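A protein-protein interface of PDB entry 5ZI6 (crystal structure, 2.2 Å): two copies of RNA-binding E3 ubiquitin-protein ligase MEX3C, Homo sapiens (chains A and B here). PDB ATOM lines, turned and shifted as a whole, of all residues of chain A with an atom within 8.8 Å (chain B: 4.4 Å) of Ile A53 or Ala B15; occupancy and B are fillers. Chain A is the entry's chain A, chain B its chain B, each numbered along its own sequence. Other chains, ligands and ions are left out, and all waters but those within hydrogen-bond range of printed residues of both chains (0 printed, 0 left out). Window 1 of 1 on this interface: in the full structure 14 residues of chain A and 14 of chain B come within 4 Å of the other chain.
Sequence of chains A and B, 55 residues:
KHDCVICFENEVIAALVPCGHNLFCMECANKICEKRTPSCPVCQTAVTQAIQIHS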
ATOM      1  N   VAL A  12     -34.362  -3.068  -4.526  1.00  0.00           N
ATOM      2  CA  VAL A  12     -32.995  -2.627  -4.309  1.00  0.00           C
ATOM      3  C   VAL A  12     -32.099  -3.341  -5.312  1.00  0.00           C
ATOM      4  O   VAL A  12     -32.095  -4.575  -5.407  1.00  0.00           O
ATOM      5  CB  VAL A  12     -32.572  -2.892  -2.855  1.00  0.00           C
ATOM      6  CG1 VAL A  12     -31.056  -2.692  -2.665  1.00  0.00           C
ATOM      7  CG2 VAL A  12     -33.353  -1.982  -1.917  1.00  0.00           C
ATOM      8  N   ILE A  13     -31.315  -2.575  -6.056  1.00  0.00           N
ATOM      9  CA  ILE A  13     -30.488  -3.168  -7.094  1.00  0.00           C
ATOM     10  C   ILE A  13     -29.091  -2.567  -7.059  1.00  0.00           C
ATOM     11  O   ILE A  13     -28.128  -3.196  -7.510  1.00  0.00           O
ATOM     12  CB  ILE A  13     -31.141  -2.928  -8.479  1.00  0.00           C
ATOM     13  CG1 ILE A  13     -32.121  -4.030  -8.870  1.00  0.00           C
ATOM     14  CG2 ILE A  13     -30.131  -2.650  -9.557  1.00  0.00           C
ATOM     15  CD1 ILE A  13     -33.380  -4.034  -8.089  1.00  0.00           C
ATOM     16  N   ALA A  14     -28.953  -1.388  -6.455  1.00  0.00           N
ATOM     17  CA  ALA A  14     -27.753  -0.579  -6.632  1.00  0.00           C
ATOM     18  C   ALA A  14     -27.200  -0.126  -5.293  1.00  0.00           C
ATOM     19  O   ALA A  14     -27.932  -0.034  -4.305  1.00  0.00           O
ATOM     20  CB  ALA A  14     -28.029   0.641  -7.505  1.00  0.00           C
ATOM     21  N   ALA A  15     -25.890   0.147  -5.274  1.00  0.00           N
ATOM     22  CA  ALA A  15     -25.205   0.712  -4.116  1.00  0.00           C
ATOM     23  C   ALA A  15     -24.423   1.958  -4.527  1.00  0.00           C
ATOM     24  O   ALA A  15     -24.045   2.120  -5.694  1.00  0.00           O
ATOM     25  CB  ALA A  15     -24.253  -0.301  -3.472  1.00  0.00           C
ATOM     26  N   LEU A  16     -24.203   2.854  -3.562  1.00  0.00           N
ATOM     27  CA  LEU A  16     -23.394   4.041  -3.813  1.00  0.00           C
ATOM     28  C   LEU A  16     -21.932   3.826  -3.418  1.00  0.00           C
ATOM     29  O   LEU A  16     -21.613   3.085  -2.481  1.00  0.00           O
ATOM     30  CB  LEU A  16     -23.963   5.240  -3.063  1.00  0.00           C
ATOM     31  CG  LEU A  16     -25.449   5.523  -3.277  1.00  0.00           C
ATOM     32  CD1 LEU A  16     -25.892   6.682  -2.376  1.00  0.00           C
ATOM     33  CD2 LEU A  16     -25.742   5.848  -4.734  1.00  0.00           C
ATOM     34  N   VAL A  17     -21.045   4.493  -4.145  1.00  0.00           N
ATOM     35  CA  VAL A  17     -19.611   4.437  -3.907  1.00  0.00           C
ATOM     36  C   VAL A  17     -19.143   5.792  -3.439  1.00  0.00           C
ATOM     37  O   VAL A  17     -19.528   6.808  -4.025  1.00  0.00           O
ATOM     38  CB  VAL A  17     -18.855   4.024  -5.168  1.00  0.00           C
ATOM     39  CG1 VAL A  17     -17.361   3.885  -4.893  1.00  0.00           C
ATOM     40  CG2 VAL A  17     -19.438   2.719  -5.715  1.00  0.00           C
ATOM     41  N   PRO A  18     -18.309   5.825  -2.381  1.00  0.00           N
ATOM     42  CA  PRO A  18     -17.759   4.660  -1.681  1.00  0.00           C
ATOM     43  C   PRO A  18     -18.479   4.218  -0.402  1.00  0.00           C
ATOM     44  O   PRO A  18     -18.023   3.232   0.161  1.00  0.00           O
ATOM     45  CB  PRO A  18     -16.346   5.136  -1.338  1.00  0.00           C
ATOM     46  CG  PRO A  18     -16.562   6.566  -0.976  1.00  0.00           C
ATOM     47  CD  PRO A  18     -17.678   7.068  -1.905  1.00  0.00           C
ATOM     48  N   GLY A  20     -21.069   2.528   0.141  1.00  0.00           N
ATOM     49  CA  GLY A  20     -21.535   1.155   0.038  1.00  0.00           C
ATOM     50  C   GLY A  20     -22.979   0.940   0.443  1.00  0.00           C
ATOM     51  O   GLY A  20     -23.409  -0.216   0.582  1.00  0.00           O
ATOM     52  N   HIS A  21     -23.743   2.005   0.652  1.00  0.00           N
ATOM     53  CA  HIS A  21     -25.146   1.832   0.997  1.00  0.00           C
ATOM     54  C   HIS A  21     -25.893   1.228  -0.182  1.00  0.00           C
ATOM     55  O   HIS A  21     -25.853   1.755  -1.300  1.00  0.00           O
ATOM     56  CB  HIS A  21     -25.778   3.146   1.457  1.00  0.00           C
ATOM     57  CG  HIS A  21     -25.630   3.367   2.932  1.00  0.00           C
ATOM     58  ND1 HIS A  21     -24.962   4.448   3.468  1.00  0.00           N
ATOM     59  CD2 HIS A  21     -25.998   2.593   3.981  1.00  0.00           C
ATOM     60  CE1 HIS A  21     -24.950   4.347   4.783  1.00  0.00           C
ATOM     61  NE2 HIS A  21     -25.570   3.229   5.120  1.00  0.00           N
ATOM     62  N   ASN A  22     -26.500   0.075   0.070  1.00  0.00           N
ATOM     63  CA  ASN A  22     -27.113  -0.770  -0.940  1.00  0.00           C
ATOM     64  C   ASN A  22     -28.604  -0.805  -0.635  1.00  0.00           C
ATOM     65  O   ASN A  22     -29.136  -1.796  -0.124  1.00  0.00           O
ATOM     66  CB  ASN A  22     -26.439  -2.183  -0.900  1.00  0.00           C
ATOM     67  CG  ASN A  22     -27.064  -3.202  -1.856  1.00  0.00           C
ATOM     68  OD1 ASN A  22     -27.516  -2.880  -2.963  1.00  0.00           O
ATOM     69  ND2 ASN A  22     -27.070  -4.451  -1.427  1.00  0.00           N
ATOM     70  N   LEU A  23     -29.273   0.327  -0.944  1.00  0.00           N
ATOM     71  CA  LEU A  23     -30.641   0.593  -0.522  1.00  0.00           C
ATOM     72  C   LEU A  23     -31.462   1.263  -1.620  1.00  0.00           C
ATOM     73  O   LEU A  23     -32.471   1.915  -1.319  1.00  0.00           O
ATOM     74  CB  LEU A  23     -30.652   1.485   0.724  1.00  0.00           C
ATOM     75  CG  LEU A  23     -30.023   0.849   1.954  1.00  0.00           C
ATOM     76  CD1 LEU A  23     -29.806   1.866   3.084  1.00  0.00           C
ATOM     77  CD2 LEU A  23     -30.922  -0.269   2.413  1.00  0.00           C
ATOM     78  N   PHE A  24     -31.035   1.172  -2.870  1.00  0.00           N
ATOM     79  CA  PHE A  24     -31.601   1.998  -3.916  1.00  0.00           C
ATOM     80  C   PHE A  24     -31.920   1.147  -5.141  1.00  0.00           C
ATOM     81  O   PHE A  24     -31.209   0.186  -5.458  1.00  0.00           O
ATOM     82  CB  PHE A  24     -30.629   3.147  -4.286  1.00  0.00           C
ATOM     83  CG  PHE A  24     -30.065   3.865  -3.082  1.00  0.00           C
ATOM     84  CD1 PHE A  24     -30.827   4.789  -2.391  1.00  0.00           C
ATOM     85  CD2 PHE A  24     -28.788   3.572  -2.615  1.00  0.00           C
ATOM     86  CE1 PHE A  24     -30.320   5.438  -1.256  1.00  0.00           C
ATOM     87  CE2 PHE A  24     -28.272   4.213  -1.485  1.00  0.00           C
ATOM     88  CZ  PHE A  24     -29.037   5.147  -0.805  1.00  0.00           C
ATOM     89  N   MET A  26     -32.041   1.339  -9.297  1.00  0.00           N
ATOM     90  CA  MET A  26     -31.057   1.995 -10.147  1.00  0.00           C
ATOM     91  C   MET A  26     -31.529   3.385 -10.570  1.00  0.00           C
ATOM     92  O   MET A  26     -30.703   4.285 -10.738  1.00  0.00           O
ATOM     93  CB  MET A  26     -30.719   1.127 -11.357  1.00  0.00           C
ATOM     94  CG  MET A  26     -29.388   1.509 -12.044  1.00  0.00           C
ATOM     95  SD  MET A  26     -27.866   1.159 -11.105  1.00  0.00           S
ATOM     96  CE  MET A  26     -26.702   2.356 -11.770  1.00  0.00           C
ATOM     97  N   ALA A  50     -22.467   5.171  -8.834  1.00  0.00           N
ATOM     98  CA  ALA A  50     -23.514   4.225  -8.475  1.00  0.00           C
ATOM     99  C   ALA A  50     -23.347   2.985  -9.338  1.00  0.00           C
ATOM    100  O   ALA A  50     -23.097   3.109 -10.536  1.00  0.00           O
ATOM    101  CB  ALA A  50     -24.887   4.840  -8.716  1.00  0.00           C
ATOM    102  N   ILE A  51     -23.444   1.794  -8.742  1.00  0.00           N
ATOM    103  CA  ILE A  51     -23.293   0.555  -9.497  1.00  0.00           C
ATOM    104  C   ILE A  51     -24.407  -0.431  -9.157  1.00  0.00           C
ATOM    105  O   ILE A  51     -24.927  -0.464  -8.036  1.00  0.00           O
ATOM    106  CB  ILE A  51     -21.911  -0.099  -9.265  1.00  0.00           C
ATOM    107  CG1 ILE A  51     -21.746  -0.556  -7.802  1.00  0.00           C
ATOM    108  CG2 ILE A  51     -20.806   0.843  -9.708  1.00  0.00           C
ATOM    109  CD1 ILE A  51     -20.523  -1.374  -7.558  1.00  0.00           C
ATOM    110  N   GLN A  52     -24.750  -1.271 -10.129  1.00  0.00           N
ATOM    111  CA  GLN A  52     -25.626  -2.388  -9.831  1.00  0.00           C
ATOM    112  C   GLN A  52     -24.867  -3.459  -9.065  1.00  0.00           C
ATOM    113  O   GLN A  52     -23.730  -3.796  -9.400  1.00  0.00           O
ATOM    114  CB  GLN A  52     -26.200  -2.984 -11.112  1.00  0.00           C
ATOM    115  CG  GLN A  52     -27.102  -4.177 -10.809  1.00  0.00           C
ATOM    116  CD  GLN A  52     -27.881  -4.680 -12.011  1.00  0.00           C
ATOM    117  OE1 GLN A  52     -28.054  -3.967 -12.999  1.00  0.00           O
ATOM    118  NE2 GLN A  52     -28.334  -5.928 -11.936  1.00  0.00           N
ATOM    119  N   ILE A  53     -25.488  -3.985  -8.021  1.00  0.00           N
ATOM    120  CA  ILE A  53     -24.872  -5.013  -7.188  1.00  0.00           C
ATOM    121  C   ILE A  53     -25.399  -6.376  -7.620  1.00  0.00           C
ATOM    122  O   ILE A  53     -26.612  -6.553  -7.785  1.00  0.00           O
ATOM    123  CB  ILE A  53     -25.143  -4.751  -5.700  1.00  0.00           C
ATOM    124  CG1 ILE A  53     -24.492  -3.434  -5.269  1.00  0.00           C
ATOM    125  CG2 ILE A  53     -24.534  -5.847  -4.872  1.00  0.00           C
ATOM    126  CD1 ILE A  53     -22.991  -3.388  -5.437  1.00  0.00           C
ATOM    127  N   HIS A  54     -24.500  -7.346  -7.764  1.00  0.00           N
ATOM    128  CA  HIS A  54     -24.860  -8.710  -8.149  1.00  0.00           C
ATOM    129  C   HIS A  54     -24.519  -9.654  -7.006  1.00  0.00           C
ATOM    130  O   HIS A  54     -23.341  -9.933  -6.746  1.00  0.00           O
ATOM    131  CB  HIS A  54     -24.127  -9.152  -9.419  1.00  0.00           C
ATOM    132  CG  HIS A  54     -24.502  -8.372 -10.635  1.00  0.00           C
ATOM    133  ND1 HIS A  54     -23.686  -7.400 -11.182  1.00  0.00           N
ATOM    134  CD2 HIS A  54     -25.618  -8.409 -11.401  1.00  0.00           C
ATOM    135  CE1 HIS A  54     -24.282  -6.880 -12.241  1.00  0.00           C
ATOM    136  NE2 HIS A  54     -25.458  -7.469 -12.390  1.00  0.00           N
ATOM    137  N   SER A  55     -25.543 -10.176  -6.356  1.00  0.00           N
ATOM    138  CA  SER A  55     -25.336 -11.079  -5.240  1.00  0.00           C
ATOM    139  C   SER A  55     -25.767 -12.480  -5.626  1.00  0.00           C
ATOM    140  O   SER A  55     -25.961 -13.321  -4.752  1.00  0.00           O
ATOM    141  CB  SER A  55     -26.112 -10.604  -4.007  1.00  0.00           C
ATOM    142  OG  SER A  55     -25.713  -9.296  -3.621  1.00  0.00           O
ATOM    143  N   ALA B  14     -18.608  -7.556   1.049  1.00  0.00           N
ATOM    144  CA  ALA B  14     -17.908  -6.642   0.169  1.00  0.00           C
ATOM    145  C   ALA B  14     -18.315  -6.876  -1.281  1.00  0.00           C
ATOM    146  O   ALA B  14     -18.625  -8.001  -1.685  1.00  0.00           O
ATOM    147  CB  ALA B  14     -16.397  -6.799   0.308  1.00  0.00           C
ATOM    148  N   ALA B  15     -18.297  -5.798  -2.065  1.00  0.00           N
ATOM    149  CA  ALA B  15     -18.527  -5.863  -3.504  1.00  0.00           C
ATOM    150  C   ALA B  15     -17.382  -5.160  -4.208  1.00  0.00           C
ATOM    151  O   ALA B  15     -16.817  -4.201  -3.680  1.00  0.00           O
ATOM    152  CB  ALA B  15     -19.841  -5.193  -3.919  1.00  0.00           C
ATOM    153  N   LEU B  16     -17.076  -5.613  -5.417  1.00  0.00           N
ATOM    154  CA  LEU B  16     -16.038  -5.008  -6.229  1.00  0.00           C
ATOM    155  C   LEU B  16     -16.658  -3.970  -7.147  1.00  0.00           C
ATOM    156  O   LEU B  16     -17.821  -4.074  -7.538  1.00  0.00           O
ATOM    157  CB  LEU B  16     -15.294  -6.067  -7.044  1.00  0.00           C
ATOM    158  CG  LEU B  16     -14.758  -7.198  -6.178  1.00  0.00           C
ATOM    159  CD1 LEU B  16     -14.151  -8.295  -7.031  1.00  0.00           C
ATOM    160  CD2 LEU B  16     -13.727  -6.637  -5.202  1.00  0.00           C
ATOM    161  N   VAL B  17     -15.878  -2.943  -7.447  1.00  0.00           N
ATOM    162  CA  VAL B  17     -16.293  -1.826  -8.289  1.00  0.00           C
ATOM    163  C   VAL B  17     -15.407  -1.896  -9.509  1.00  0.00           C
ATOM    164  O   VAL B  17     -14.221  -2.110  -9.370  1.00  0.00           O
ATOM    165  CB  VAL B  17     -16.153  -0.486  -7.519  1.00  0.00           C
ATOM    166  CG1 VAL B  17     -16.697   0.726  -8.313  1.00  0.00           C
ATOM    167  CG2 VAL B  17     -16.821  -0.602  -6.172  1.00  0.00           C
ATOM    168  N   GLY B  20     -19.562  -4.895  -9.526  1.00  0.00           N
ATOM    169  CA  GLY B  20     -20.618  -5.016  -8.531  1.00  0.00           C
ATOM    170  C   GLY B  20     -20.837  -6.410  -7.968  1.00  0.00           C
ATOM    171  O   GLY B  20     -21.839  -6.637  -7.275  1.00  0.00           O
ATOM    172  N   HIS B  21     -19.954  -7.348  -8.242  1.00  0.00           N
ATOM    173  CA  HIS B  21     -20.105  -8.685  -7.686  1.00  0.00           C
ATOM    174  C   HIS B  21     -19.882  -8.668  -6.188  1.00  0.00           C
ATOM    175  O   HIS B  21     -18.832  -8.243  -5.705  1.00  0.00           O
ATOM    176  CB  HIS B  21     -19.163  -9.660  -8.373  1.00  0.00           C
ATOM    177  CG  HIS B  21     -19.749 -10.270  -9.604  1.00  0.00           C
ATOM    178  ND1 HIS B  21     -19.199 -10.092 -10.857  1.00  0.00           N
ATOM    179  CD2 HIS B  21     -20.827 -11.072  -9.770  1.00  0.00           C
ATOM    180  CE1 HIS B  21     -19.918 -10.756 -11.743  1.00  0.00           C
ATOM    181  NE2 HIS B  21     -20.914 -11.356 -11.111  1.00  0.00           N
ATOM    182  N   ASN B  22     -20.885  -9.138  -5.464  1.00  0.00           N
ATOM    183  CA  ASN B  22     -20.992  -9.052  -4.028  1.00  0.00           C
ATOM    184  C   ASN B  22     -20.921 -10.485  -3.502  1.00  0.00           C
ATOM    185  O   ASN B  22     -21.924 -11.096  -3.139  1.00  0.00           O
ATOM    186  CB  ASN B  22     -22.276  -8.356  -3.702  1.00  0.00           C
ATOM    187  CG  ASN B  22     -22.550  -8.271  -2.215  1.00  0.00           C
ATOM    188  OD1 ASN B  22     -23.717  -8.188  -1.799  1.00  0.00           O
ATOM    189  ND2 ASN B  22     -21.490  -8.292  -1.401  1.00  0.00           N
ATOM    190  N   ALA B  50     -12.735  -1.881  -3.793  1.00  0.00           N
ATOM    191  CA  ALA B  50     -13.672  -2.784  -3.154  1.00  0.00           C
ATOM    192  C   ALA B  50     -14.410  -1.981  -2.106  1.00  0.00           C
ATOM    193  O   ALA B  50     -13.829  -1.087  -1.496  1.00  0.00           O
ATOM    194  CB  ALA B  50     -12.976  -3.975  -2.514  1.00  0.00           C
ATOM    195  N   ILE B  51     -15.704  -2.212  -1.955  1.00  0.00           N
ATOM    196  CA  ILE B  51     -16.424  -1.481  -0.924  1.00  0.00           C
ATOM    197  C   ILE B  51     -17.150  -2.475  -0.038  1.00  0.00           C
ATOM    198  O   ILE B  51     -17.562  -3.554  -0.474  1.00  0.00           O
ATOM    199  CB  ILE B  51     -17.410  -0.438  -1.494  1.00  0.00           C
ATOM    200  CG1 ILE B  51     -18.521  -1.118  -2.280  1.00  0.00           C
ATOM    201  CG2 ILE B  51     -16.685   0.552  -2.367  1.00  0.00           C
ATOM    202  CD1 ILE B  51     -19.626  -0.161  -2.649  1.00  0.00           C
ATOM    203  N   ILE B  53     -20.466  -3.455   1.799  1.00  0.00           N
ATOM    204  CA  ILE B  53     -21.868  -3.237   1.475  1.00  0.00           C
ATOM    205  C   ILE B  53     -22.671  -3.056   2.754  1.00  0.00           C
ATOM    206  O   ILE B  53     -22.574  -3.863   3.682  1.00  0.00           O
ATOM    207  CB  ILE B  53     -22.425  -4.410   0.655  1.00  0.00           C
ATOM    208  CG1 ILE B  53     -21.758  -4.455  -0.724  1.00  0.00           C
ATOM    209  CG2 ILE B  53     -23.958  -4.357   0.637  1.00  0.00           C
ATOM    210  CD1 ILE B  53     -21.939  -3.182  -1.526  1.00  0.00           C
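N of His A54 sits at hydrogen-bond distance from O of Gly B20 (2.8 Å).
The backbone carbonyl oxygen (O) of His A54 lies within hydrogen-bond range of the backbone NH (N) of Asn B22, at 2.9 Å.
OG of Ser A55 lies within hydrogen-bond range of OD1 of Asn B22 (2.9 Å).
The backbone carbonyl oxygen (O) of Ile A13 lies within hydrogen-bond range of the backbone NH (N) of Ile A53 (2.8 Å).
The side-chain amide oxygen (OD1) of Asn A22 lies close to the backbone carbonyl oxygen (O) of Ala A14.
The backbone NH (N) of Leu A16 sits at hydrogen-bond distance from the backbone carbonyl oxygen (O) of His A21, 3.0 Å away.
NE2 of Gln A52 lies within hydrogen-bond range of NE2 of His A54, at 3.3 Å.
The backbone carbonyl oxygen of Ala B14 lies within hydrogen-bond range of the side-chain amide nitrogen of Asn B22 (2.9 Å).
O of His B21 lies within hydrogen-bond range of N of Leu B16, 3.2 Å away.
CD1 of Ile B51 touches O of Leu A16, at 3.8 Å.
Ile B51 touches Pro A18.
Ile B51 touches Gly A20 (CD1 to CA, 3.5 Å).
Ile B53 touches Gly A20 (CA to O, 3.5 Å).
O of Leu B16 touches CD1 of Ile A51, 3.8 Å away.
Ile A51 touches Gly B20.
Gly B20 touches Gln A52.
Ala B15 touches Ile A53 (CB to CD1, 3.9 Å).
Ile A53 touches Gly B20.
Ile A53 touches Asn B22.
Ile A53 touches just these residues of chain B: Ala B15 (3.9 Å), Gly B20 (3.4 Å) and Asn B22 (3.6 Å).
Of chain A, only Ile A53 comes within 4 Å of Ala B15.
No residue of chain A comes within 4 Å of Ala B14.
Printed residues of chain B within 4 Å of Ser A55: Asn B22.
Printed residues of chain B within 4 Å of Leu A16: Ile B51.
The nearest residue of chain B that does not touch Ile A53 is Ile B53 (4.1 Å).
The nearest printed residue of chain B that does not touch Pro A18 is Ala B50 (6.2 Å).
Along chain A the printed residues that touch a printed residue of chain B span positions 16 to 55.
Hydrophobic or aromatic side chains of chain B within 4 Å of the printed part of chain A: Ala B15, His B21, Ile B51 and Ile B53.
Among the printed residues, 15 pairs touch across the chains.
Among the printed residues, no Asp or Glu carboxylate lies within 4 Å of a Lys or Arg side-chain nitrogen of the other chain.
Leu A16 touches Ile B51, and with the chains exchanged Ile A51 touches Leu B16.
Gly A20 touches Ile B51, and with the chains exchanged Ile A51 touches Gly B20.
Gly A20 touches Ile B53, and with the chains exchanged Ile A53 touches Gly B20.
Ile A53 touches Ala B15, but with the chains exchanged Ala A15 does not touch Ile B53 (4.2 Å).
Positions printed for both chains: 14, 15, 16, 17, 20, 21, 22, 50, 51 and 53.
Of the 15 pairs that touch across the chains among the printed residues, 8 have their exchanged pair printed and touching as well.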
